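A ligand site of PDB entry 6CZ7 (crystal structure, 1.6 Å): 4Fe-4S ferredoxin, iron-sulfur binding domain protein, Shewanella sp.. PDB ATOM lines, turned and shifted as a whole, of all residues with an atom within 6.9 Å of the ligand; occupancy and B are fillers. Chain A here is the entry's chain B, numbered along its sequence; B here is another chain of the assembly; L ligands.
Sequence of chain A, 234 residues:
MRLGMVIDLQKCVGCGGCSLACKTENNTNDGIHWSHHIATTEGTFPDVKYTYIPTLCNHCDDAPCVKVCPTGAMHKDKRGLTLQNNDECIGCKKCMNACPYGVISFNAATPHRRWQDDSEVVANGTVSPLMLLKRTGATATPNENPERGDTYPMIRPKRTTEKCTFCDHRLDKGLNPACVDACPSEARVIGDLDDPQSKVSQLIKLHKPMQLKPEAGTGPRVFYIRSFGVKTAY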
ATOM      1  N   ILE A   7      22.165 -21.870  -0.188  1.00  0.00           N
ATOM      2  CA  ILE A   7      20.879 -22.457   0.140  1.00  0.00           C
ATOM      3  C   ILE A   7      20.021 -21.390   0.777  1.00  0.00           C
ATOM      4  O   ILE A   7      20.386 -20.823   1.827  1.00  0.00           O
ATOM      5  CB  ILE A   7      21.029 -23.685   1.039  1.00  0.00           C
ATOM      6  CG1 ILE A   7      21.833 -24.758   0.293  1.00  0.00           C
ATOM      7  CG2 ILE A   7      19.654 -24.204   1.449  1.00  0.00           C
ATOM      8  CD1 ILE A   7      22.144 -26.001   1.133  1.00  0.00           C
ATOM      9  N   ASP A   8      18.857 -21.153   0.196  1.00  0.00           N
ATOM     10  CA  ASP A   8      17.917 -20.140   0.655  1.00  0.00           C
ATOM     11  C   ASP A   8      16.943 -20.768   1.645  1.00  0.00           C
ATOM     12  O   ASP A   8      16.029 -21.497   1.236  1.00  0.00           O
ATOM     13  CB  ASP A   8      17.187 -19.560  -0.562  1.00  0.00           C
ATOM     14  CG  ASP A   8      16.291 -18.421  -0.214  1.00  0.00           C
ATOM     15  OD1 ASP A   8      15.820 -18.334   0.938  1.00  0.00           O
ATOM     16  OD2 ASP A   8      16.027 -17.618  -1.130  1.00  0.00           O
ATOM     17  N   LYS A  11      13.140 -20.191   1.124  1.00  0.00           N
ATOM     18  CA  LYS A  11      12.540 -21.052   0.113  1.00  0.00           C
ATOM     19  C   LYS A  11      12.432 -22.496   0.581  1.00  0.00           C
ATOM     20  O   LYS A  11      11.507 -23.212   0.198  1.00  0.00           O
ATOM     21  CB  LYS A  11      13.359 -20.990  -1.175  1.00  0.00           C
ATOM     22  CG  LYS A  11      13.231 -19.683  -1.964  1.00  0.00           C
ATOM     23  CD  LYS A  11      14.194 -19.673  -3.160  1.00  0.00           C
ATOM     24  CE  LYS A  11      13.914 -18.520  -4.129  1.00  0.00           C
ATOM     25  NZ  LYS A  11      12.752 -18.801  -5.015  1.00  0.00           N
ATOM     26  N   CYS A  12      13.382 -22.944   1.409  1.00  0.00           N
ATOM     27  CA  CYS A  12      13.403 -24.340   1.827  1.00  0.00           C
ATOM     28  C   CYS A  12      12.168 -24.686   2.653  1.00  0.00           C
ATOM     29  O   CYS A  12      11.773 -23.928   3.539  1.00  0.00           O
ATOM     30  CB  CYS A  12      14.682 -24.613   2.623  1.00  0.00           C
ATOM     31  SG  CYS A  12      14.865 -26.307   3.197  1.00  0.00           S
ATOM     32  N   VAL A  13      11.559 -25.837   2.344  1.00  0.00           N
ATOM     33  CA  VAL A  13      10.411 -26.310   3.106  1.00  0.00           C
ATOM     34  C   VAL A  13      10.732 -27.523   3.964  1.00  0.00           C
ATOM     35  O   VAL A  13       9.837 -28.110   4.569  1.00  0.00           O
ATOM     36  CB  VAL A  13       9.189 -26.593   2.198  1.00  0.00           C
ATOM     37  CG1 VAL A  13       8.767 -25.325   1.495  1.00  0.00           C
ATOM     38  CG2 VAL A  13       9.486 -27.698   1.188  1.00  0.00           C
ATOM     39  N   GLY A  14      12.003 -27.923   4.029  1.00  0.00           N
ATOM     40  CA  GLY A  14      12.422 -28.989   4.920  1.00  0.00           C
ATOM     41  C   GLY A  14      11.893 -30.354   4.560  1.00  0.00           C
ATOM     42  O   GLY A  14      11.614 -31.153   5.458  1.00  0.00           O
ATOM     43  N   CYS A  15      11.755 -30.640   3.264  1.00  0.00           N
ATOM     44  CA  CYS A  15      11.075 -31.839   2.787  1.00  0.00           C
ATOM     45  C   CYS A  15      12.003 -33.035   2.604  1.00  0.00           C
ATOM     46  O   CYS A  15      11.512 -34.170   2.522  1.00  0.00           O
ATOM     47  CB  CYS A  15      10.374 -31.562   1.451  1.00  0.00           C
ATOM     48  SG  CYS A  15      11.460 -31.187   0.014  1.00  0.00           S
ATOM     49  N   GLY A  16      13.317 -32.820   2.516  1.00  0.00           N
ATOM     50  CA  GLY A  16      14.237 -33.903   2.270  1.00  0.00           C
ATOM     51  C   GLY A  16      14.322 -34.373   0.839  1.00  0.00           C
ATOM     52  O   GLY A  16      14.949 -35.411   0.580  1.00  0.00           O
ATOM     53  N   GLY A  17      13.714 -33.654  -0.104  1.00  0.00           N
ATOM     54  CA  GLY A  17      13.753 -34.095  -1.490  1.00  0.00           C
ATOM     55  C   GLY A  17      15.160 -34.118  -2.041  1.00  0.00           C
ATOM     56  O   GLY A  17      15.513 -35.006  -2.823  1.00  0.00           O
ATOM     57  N   CYS A  18      15.979 -33.160  -1.621  1.00  0.00           N
ATOM     58  CA  CYS A  18      17.390 -33.131  -1.995  1.00  0.00           C
ATOM     59  C   CYS A  18      18.101 -34.393  -1.521  1.00  0.00           C
ATOM     60  O   CYS A  18      18.857 -35.016  -2.275  1.00  0.00           O
ATOM     61  CB  CYS A  18      18.028 -31.890  -1.406  1.00  0.00           C
ATOM     62  SG  CYS A  18      17.579 -31.622   0.313  1.00  0.00           S
ATOM     63  N   SER A  19      17.838 -34.795  -0.275  1.00  0.00           N
ATOM     64  CA  SER A  19      18.517 -35.957   0.282  1.00  0.00           C
ATOM     65  C   SER A  19      18.060 -37.237  -0.395  1.00  0.00           C
ATOM     66  O   SER A  19      18.857 -38.149  -0.617  1.00  0.00           O
ATOM     67  CB  SER A  19      18.273 -36.032   1.779  1.00  0.00           C
ATOM     68  OG  SER A  19      18.738 -34.835   2.381  1.00  0.00           O
ATOM     69  N   SER A  35      23.658 -36.174   1.485  1.00  0.00           N
ATOM     70  CA  SER A  35      22.808 -35.052   1.816  1.00  0.00           C
ATOM     71  C   SER A  35      21.989 -35.439   3.033  1.00  0.00           C
ATOM     72  O   SER A  35      21.403 -36.521   3.083  1.00  0.00           O
ATOM     73  CB  SER A  35      21.878 -34.725   0.638  1.00  0.00           C
ATOM     74  OG  SER A  35      20.889 -33.789   1.021  1.00  0.00           O
ATOM     75  N   HIS A  37      20.464 -33.331   7.009  1.00  0.00           N
ATOM     76  CA  HIS A  37      19.901 -32.104   7.531  1.00  0.00           C
ATOM     77  C   HIS A  37      20.191 -31.999   9.019  1.00  0.00           C
ATOM     78  O   HIS A  37      20.525 -32.987   9.682  1.00  0.00           O
ATOM     79  CB  HIS A  37      18.388 -32.039   7.305  1.00  0.00           C
ATOM     80  CG  HIS A  37      17.662 -33.187   7.937  1.00  0.00           C
ATOM     81  ND1 HIS A  37      17.395 -34.352   7.260  1.00  0.00           N
ATOM     82  CD2 HIS A  37      17.210 -33.372   9.199  1.00  0.00           C
ATOM     83  CE1 HIS A  37      16.767 -35.192   8.071  1.00  0.00           C
ATOM     84  NE2 HIS A  37      16.650 -34.621   9.253  1.00  0.00           N
ATOM     85  N   TYR A  52      14.775 -26.281   9.705  1.00  0.00           N
ATOM     86  CA  TYR A  52      15.445 -27.356   8.986  1.00  0.00           C
ATOM     87  C   TYR A  52      16.573 -26.740   8.188  1.00  0.00           C
ATOM     88  O   TYR A  52      16.361 -25.774   7.451  1.00  0.00           O
ATOM     89  CB  TYR A  52      14.459 -28.050   8.067  1.00  0.00           C
ATOM     90  CG  TYR A  52      14.956 -29.168   7.195  1.00  0.00           C
ATOM     91  CD1 TYR A  52      15.694 -28.914   6.051  1.00  0.00           C
ATOM     92  CD2 TYR A  52      14.590 -30.469   7.466  1.00  0.00           C
ATOM     93  CE1 TYR A  52      16.081 -29.941   5.216  1.00  0.00           C
ATOM     94  CE2 TYR A  52      14.973 -31.496   6.656  1.00  0.00           C
ATOM     95  CZ  TYR A  52      15.715 -31.235   5.532  1.00  0.00           C
ATOM     96  OH  TYR A  52      16.085 -32.279   4.720  1.00  0.00           O
ATOM     97  N   PRO A  54      19.348 -27.907   5.440  1.00  0.00           N
ATOM     98  CA  PRO A  54      19.942 -28.969   4.620  1.00  0.00           C
ATOM     99  C   PRO A  54      21.449 -28.946   4.739  1.00  0.00           C
ATOM    100  O   PRO A  54      22.063 -27.872   4.778  1.00  0.00           O
ATOM    101  CB  PRO A  54      19.492 -28.620   3.188  1.00  0.00           C
ATOM    102  CG  PRO A  54      18.431 -27.561   3.336  1.00  0.00           C
ATOM    103  CD  PRO A  54      18.716 -26.856   4.620  1.00  0.00           C
ATOM    104  N   CYS A 179      20.522 -32.837  -6.180  1.00  0.00           N
ATOM    105  CA  CYS A 179      19.785 -32.152  -5.126  1.00  0.00           C
ATOM    106  C   CYS A 179      19.345 -30.761  -5.570  1.00  0.00           C
ATOM    107  O   CYS A 179      18.300 -30.282  -5.118  1.00  0.00           O
ATOM    108  CB  CYS A 179      20.646 -32.046  -3.873  1.00  0.00           C
ATOM    109  SG  CYS A 179      22.193 -31.196  -4.134  1.00  0.00           S
ATOM    110  N   ALA A 182      16.388 -31.306  -7.757  1.00  0.00           N
ATOM    111  CA  ALA A 182      15.285 -31.917  -7.021  1.00  0.00           C
ATOM    112  C   ALA A 182      14.521 -30.921  -6.158  1.00  0.00           C
ATOM    113  O   ALA A 182      13.449 -31.267  -5.656  1.00  0.00           O
ATOM    114  CB  ALA A 182      15.832 -33.056  -6.152  1.00  0.00           C
ATOM    115  N   CYS A 183      15.039 -29.712  -5.962  1.00  0.00           N
ATOM    116  CA  CYS A 183      14.459 -28.806  -4.983  1.00  0.00           C
ATOM    117  C   CYS A 183      13.245 -28.080  -5.565  1.00  0.00           C
ATOM    118  O   CYS A 183      13.403 -27.338  -6.544  1.00  0.00           O
ATOM    119  CB  CYS A 183      15.471 -27.774  -4.532  1.00  0.00           C
ATOM    120  SG  CYS A 183      14.733 -26.640  -3.337  1.00  0.00           S
ATOM    121  N   PRO A 184      12.066 -28.230  -4.978  1.00  0.00           N
ATOM    122  CA  PRO A 184      10.882 -27.661  -5.626  1.00  0.00           C
ATOM    123  C   PRO A 184      10.889 -26.148  -5.682  1.00  0.00           C
ATOM    124  O   PRO A 184      10.264 -25.573  -6.582  1.00  0.00           O
ATOM    125  CB  PRO A 184       9.723 -28.165  -4.753  1.00  0.00           C
ATOM    126  CG  PRO A 184      10.352 -28.403  -3.422  1.00  0.00           C
ATOM    127  CD  PRO A 184      11.726 -28.939  -3.729  1.00  0.00           C
ATOM    128  N   SER A 185      11.558 -25.485  -4.749  1.00  0.00           N
ATOM    129  CA  SER A 185      11.563 -24.043  -4.650  1.00  0.00           C
ATOM    130  C   SER A 185      12.853 -23.426  -5.176  1.00  0.00           C
ATOM    131  O   SER A 185      13.051 -22.209  -5.034  1.00  0.00           O
ATOM    132  CB  SER A 185      11.369 -23.627  -3.199  1.00  0.00           C
ATOM    133  OG  SER A 185      12.401 -24.201  -2.411  1.00  0.00           O
ATOM    134  N   GLU A 186      13.709 -24.216  -5.809  1.00  0.00           N
ATOM    135  CA  GLU A 186      14.998 -23.721  -6.307  1.00  0.00           C
ATOM    136  C   GLU A 186      15.778 -23.048  -5.182  1.00  0.00           C
ATOM    137  O   GLU A 186      16.461 -22.043  -5.370  1.00  0.00           O
ATOM    138  CB  GLU A 186      14.771 -22.751  -7.470  1.00  0.00           C
ATOM    139  CG  GLU A 186      14.050 -23.360  -8.657  1.00  0.00           C
ATOM    140  CD  GLU A 186      13.975 -22.434  -9.859  1.00  0.00           C
ATOM    141  OE1 GLU A 186      14.036 -21.191  -9.675  1.00  0.00           O
ATOM    142  OE2 GLU A 186      13.837 -22.941 -10.987  1.00  0.00           O
ATOM    143  N   ALA A 187      15.684 -23.637  -3.977  1.00  0.00           N
ATOM    144  CA  ALA A 187      16.380 -23.059  -2.846  1.00  0.00           C
ATOM    145  C   ALA A 187      17.888 -23.222  -2.954  1.00  0.00           C
ATOM    146  O   ALA A 187      18.620 -22.484  -2.282  1.00  0.00           O
ATOM    147  CB  ALA A 187      15.906 -23.707  -1.543  1.00  0.00           C
ATOM    148  N   ARG A 188      18.376 -24.160  -3.762  1.00  0.00           N
ATOM    149  CA  ARG A 188      19.792 -24.486  -3.852  1.00  0.00           C
ATOM    150  C   ARG A 188      20.352 -23.987  -5.166  1.00  0.00           C
ATOM    151  O   ARG A 188      19.794 -24.282  -6.230  1.00  0.00           O
ATOM    152  CB  ARG A 188      20.012 -26.002  -3.736  1.00  0.00           C
ATOM    153  CG  ARG A 188      19.294 -26.642  -2.561  1.00  0.00           C
ATOM    154  CD  ARG A 188      19.146 -28.141  -2.695  1.00  0.00           C
ATOM    155  NE  ARG A 188      20.359 -28.912  -2.435  1.00  0.00           N
ATOM    156  CZ  ARG A 188      20.723 -29.357  -1.239  1.00  0.00           C
ATOM    157  NH1 ARG A 188      20.000 -29.069  -0.160  1.00  0.00           N
ATOM    158  NH2 ARG A 188      21.828 -30.077  -1.115  1.00  0.00           N
ATOM    159  N   PHE A 228      14.460 -19.705   7.732  1.00  0.00           N
ATOM    160  CA  PHE A 228      13.468 -20.736   7.499  1.00  0.00           C
ATOM    161  C   PHE A 228      12.109 -20.292   7.994  1.00  0.00           C
ATOM    162  O   PHE A 228      11.096 -20.488   7.313  1.00  0.00           O
ATOM    163  CB  PHE A 228      13.907 -22.015   8.226  1.00  0.00           C
ATOM    164  CG  PHE A 228      13.076 -23.207   7.880  1.00  0.00           C
ATOM    165  CD1 PHE A 228      13.377 -23.985   6.788  1.00  0.00           C
ATOM    166  CD2 PHE A 228      12.003 -23.567   8.685  1.00  0.00           C
ATOM    167  CE1 PHE A 228      12.616 -25.093   6.481  1.00  0.00           C
ATOM    168  CE2 PHE A 228      11.240 -24.670   8.386  1.00  0.00           C
ATOM    169  CZ  PHE A 228      11.538 -25.436   7.272  1.00  0.00           C
ATOM    170  N   SER B  55       8.839 -30.650  -7.443  1.00  0.00           N
ATOM    171  CA  SER B  55       8.313 -31.883  -6.911  1.00  0.00           C
ATOM    172  C   SER B  55       8.437 -31.908  -5.394  1.00  0.00           C
ATOM    173  O   SER B  55       9.377 -31.347  -4.814  1.00  0.00           O
ATOM    174  CB  SER B  55       9.065 -33.106  -7.450  1.00  0.00           C
ATOM    175  OG  SER B  55       8.526 -34.300  -6.938  1.00  0.00           O
ATOM    176  N   PRO B  57       9.059 -34.505  -2.041  1.00  0.00           N
ATOM    177  CA  PRO B  57      10.148 -35.485  -1.900  1.00  0.00           C
ATOM    178  C   PRO B  57       9.739 -36.910  -2.242  1.00  0.00           C
ATOM    179  O   PRO B  57      10.610 -37.745  -2.494  1.00  0.00           O
ATOM    180  CB  PRO B  57      10.539 -35.360  -0.420  1.00  0.00           C
ATOM    181  CG  PRO B  57       9.243 -34.938   0.255  1.00  0.00           C
ATOM    182  CD  PRO B  57       8.587 -33.997  -0.739  1.00  0.00           C
ATOM    183  N   SER B 199       4.923 -26.097  -2.444  1.00  0.00           N
ATOM    184  CA  SER B 199       6.292 -26.053  -1.934  1.00  0.00           C
ATOM    185  C   SER B 199       7.157 -25.115  -2.761  1.00  0.00           C
ATOM    186  O   SER B 199       8.051 -24.436  -2.229  1.00  0.00           O
ATOM    187  CB  SER B 199       6.929 -27.447  -1.934  1.00  0.00           C
ATOM    188  OG  SER B 199       6.263 -28.308  -1.026  1.00  0.00           O
ATOM    189  N   ARG B 686       4.635 -36.541   5.509  1.00  0.00           N
ATOM    190  CA  ARG B 686       4.956 -35.943   4.226  1.00  0.00           C
ATOM    191  C   ARG B 686       5.704 -36.906   3.323  1.00  0.00           C
ATOM    192  O   ARG B 686       5.942 -36.584   2.157  1.00  0.00           O
ATOM    193  CB  ARG B 686       5.763 -34.652   4.403  1.00  0.00           C
ATOM    194  CG  ARG B 686       7.248 -34.818   4.598  1.00  0.00           C
ATOM    195  CD  ARG B 686       7.840 -33.542   5.203  1.00  0.00           C
ATOM    196  NE  ARG B 686       7.631 -32.341   4.402  1.00  0.00           N
ATOM    197  CZ  ARG B 686       7.975 -31.119   4.784  1.00  0.00           C
ATOM    198  NH1 ARG B 686       8.551 -30.941   5.967  1.00  0.00           N
ATOM    199  NH2 ARG B 686       7.768 -30.068   3.996  1.00  0.00           N
ATOM    200  N   VAL B 705      11.760 -35.915   8.485  1.00  0.00           N
ATOM    201  CA  VAL B 705      11.385 -34.693   7.776  1.00  0.00           C
ATOM    202  C   VAL B 705       9.988 -34.258   8.193  1.00  0.00           C
ATOM    203  O   VAL B 705       9.616 -33.089   7.983  1.00  0.00           O
ATOM    204  CB  VAL B 705      11.476 -34.847   6.246  1.00  0.00           C
ATOM    205  CG1 VAL B 705      12.917 -35.085   5.826  1.00  0.00           C
ATOM    206  CG2 VAL B 705      10.558 -35.938   5.717  1.00  0.00           C
HETATM  207 FE1  LIG L   1      13.303 -29.617   0.166  1.00  0.00          FE
HETATM  208 FE2  LIG L   1      14.846 -27.666   1.304  1.00  0.00          FE
HETATM  209 FE3  LIG L   1      14.837 -27.945  -1.346  1.00  0.00          FE
HETATM  210 FE4  LIG L   1      16.024 -29.816   0.153  1.00  0.00          FE
HETATM  211  S1  LIG L   1      16.682 -27.646  -0.050  1.00  0.00           S
HETATM  212  S2  LIG L   1      14.633 -30.188  -1.610  1.00  0.00           S
HETATM  213  S3  LIG L   1      14.646 -29.823   1.978  1.00  0.00           S
HETATM  214  S4  LIG L   1      13.031 -27.389  -0.056  1.00  0.00           S
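The side-chain sulfur (SG) of Cys 12 is bound to an iron atom (FE2) of the ligand.
The side-chain sulfur (SG) of Cys 183 binds an iron atom (FE3) of the ligand (2.4 Å).
The backbone NH (N) of Cys 18 lies close to a sulfur (S2) of the ligand (3.3 Å).
The side-chain sulfur (SG) of Cys 18 is bound to an iron atom (FE4) of the ligand, at 2.4 Å.
The backbone NH (N) of Cys 15 sits close to a sulfur (S3) of the ligand, 3.3 Å away.
An iron atom (FE1) of the ligand is bound by the side-chain sulfur (SG) of Cys 15.
A sulfur (S4) of the ligand lies close to the backbone NH (N) of Val 13 (3.2 Å).
A sulfur (S3) of the ligand lies close to the backbone NH of Gly 16, at 3.3 Å.
NH1 of Arg 188 lies close to S1 of the ligand (3.6 Å).
Gly 14 touches the ligand (CA to S3, 3.8 Å).
Gly 17 touches the ligand (N to S2, 3.9 Å).
Tyr 52 touches the ligand (CE1 to S3, 3.5 Å).
Pro 54 touches the ligand.
Pro 184 touches the ligand (CD to S2, 3.8 Å).
Of the 29 residues printed, 12 come within 4 Å of the ligand.
Along chain A the residues within 4 Å of the ligand span positions 12 to 188.
The nearest printed residue that does not touch the ligand is Ser 185 (4.01 Å).
The backbone NH (N) of Gly 14 lies close to the side-chain sulfur (SG) of Cys 12 (3.4 Å).
The side-chain sulfur (SG) of Cys 183 lies close to the side-chain hydroxyl (OG) of Ser 185 (3.5 Å).
The side-chain sulfur of Cys 183 lies close to the backbone NH of Ala 187 (3.2 Å).
The side-chain sulfur (SG) of Cys 183 sits close to the backbone NH (N) of Glu 186.
The side-chain sulfur (SG) of Cys 18 sits close to the guanidinium group (NH1) of Arg 188 (3.6 Å).
The side-chain sulfur (SG) of Cys 15 lies close to the backbone NH (N) of Gly 17.
The guanidinium group (NH2) of Arg 188 lies close to the side-chain sulfur (SG) of Cys 179, at 3.2 Å.
The backbone carbonyl oxygen (O) of Gly 14 is in hydrogen-bond range of the guanidinium group (NH1) of Arg 686 of chain B (3.1 Å).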
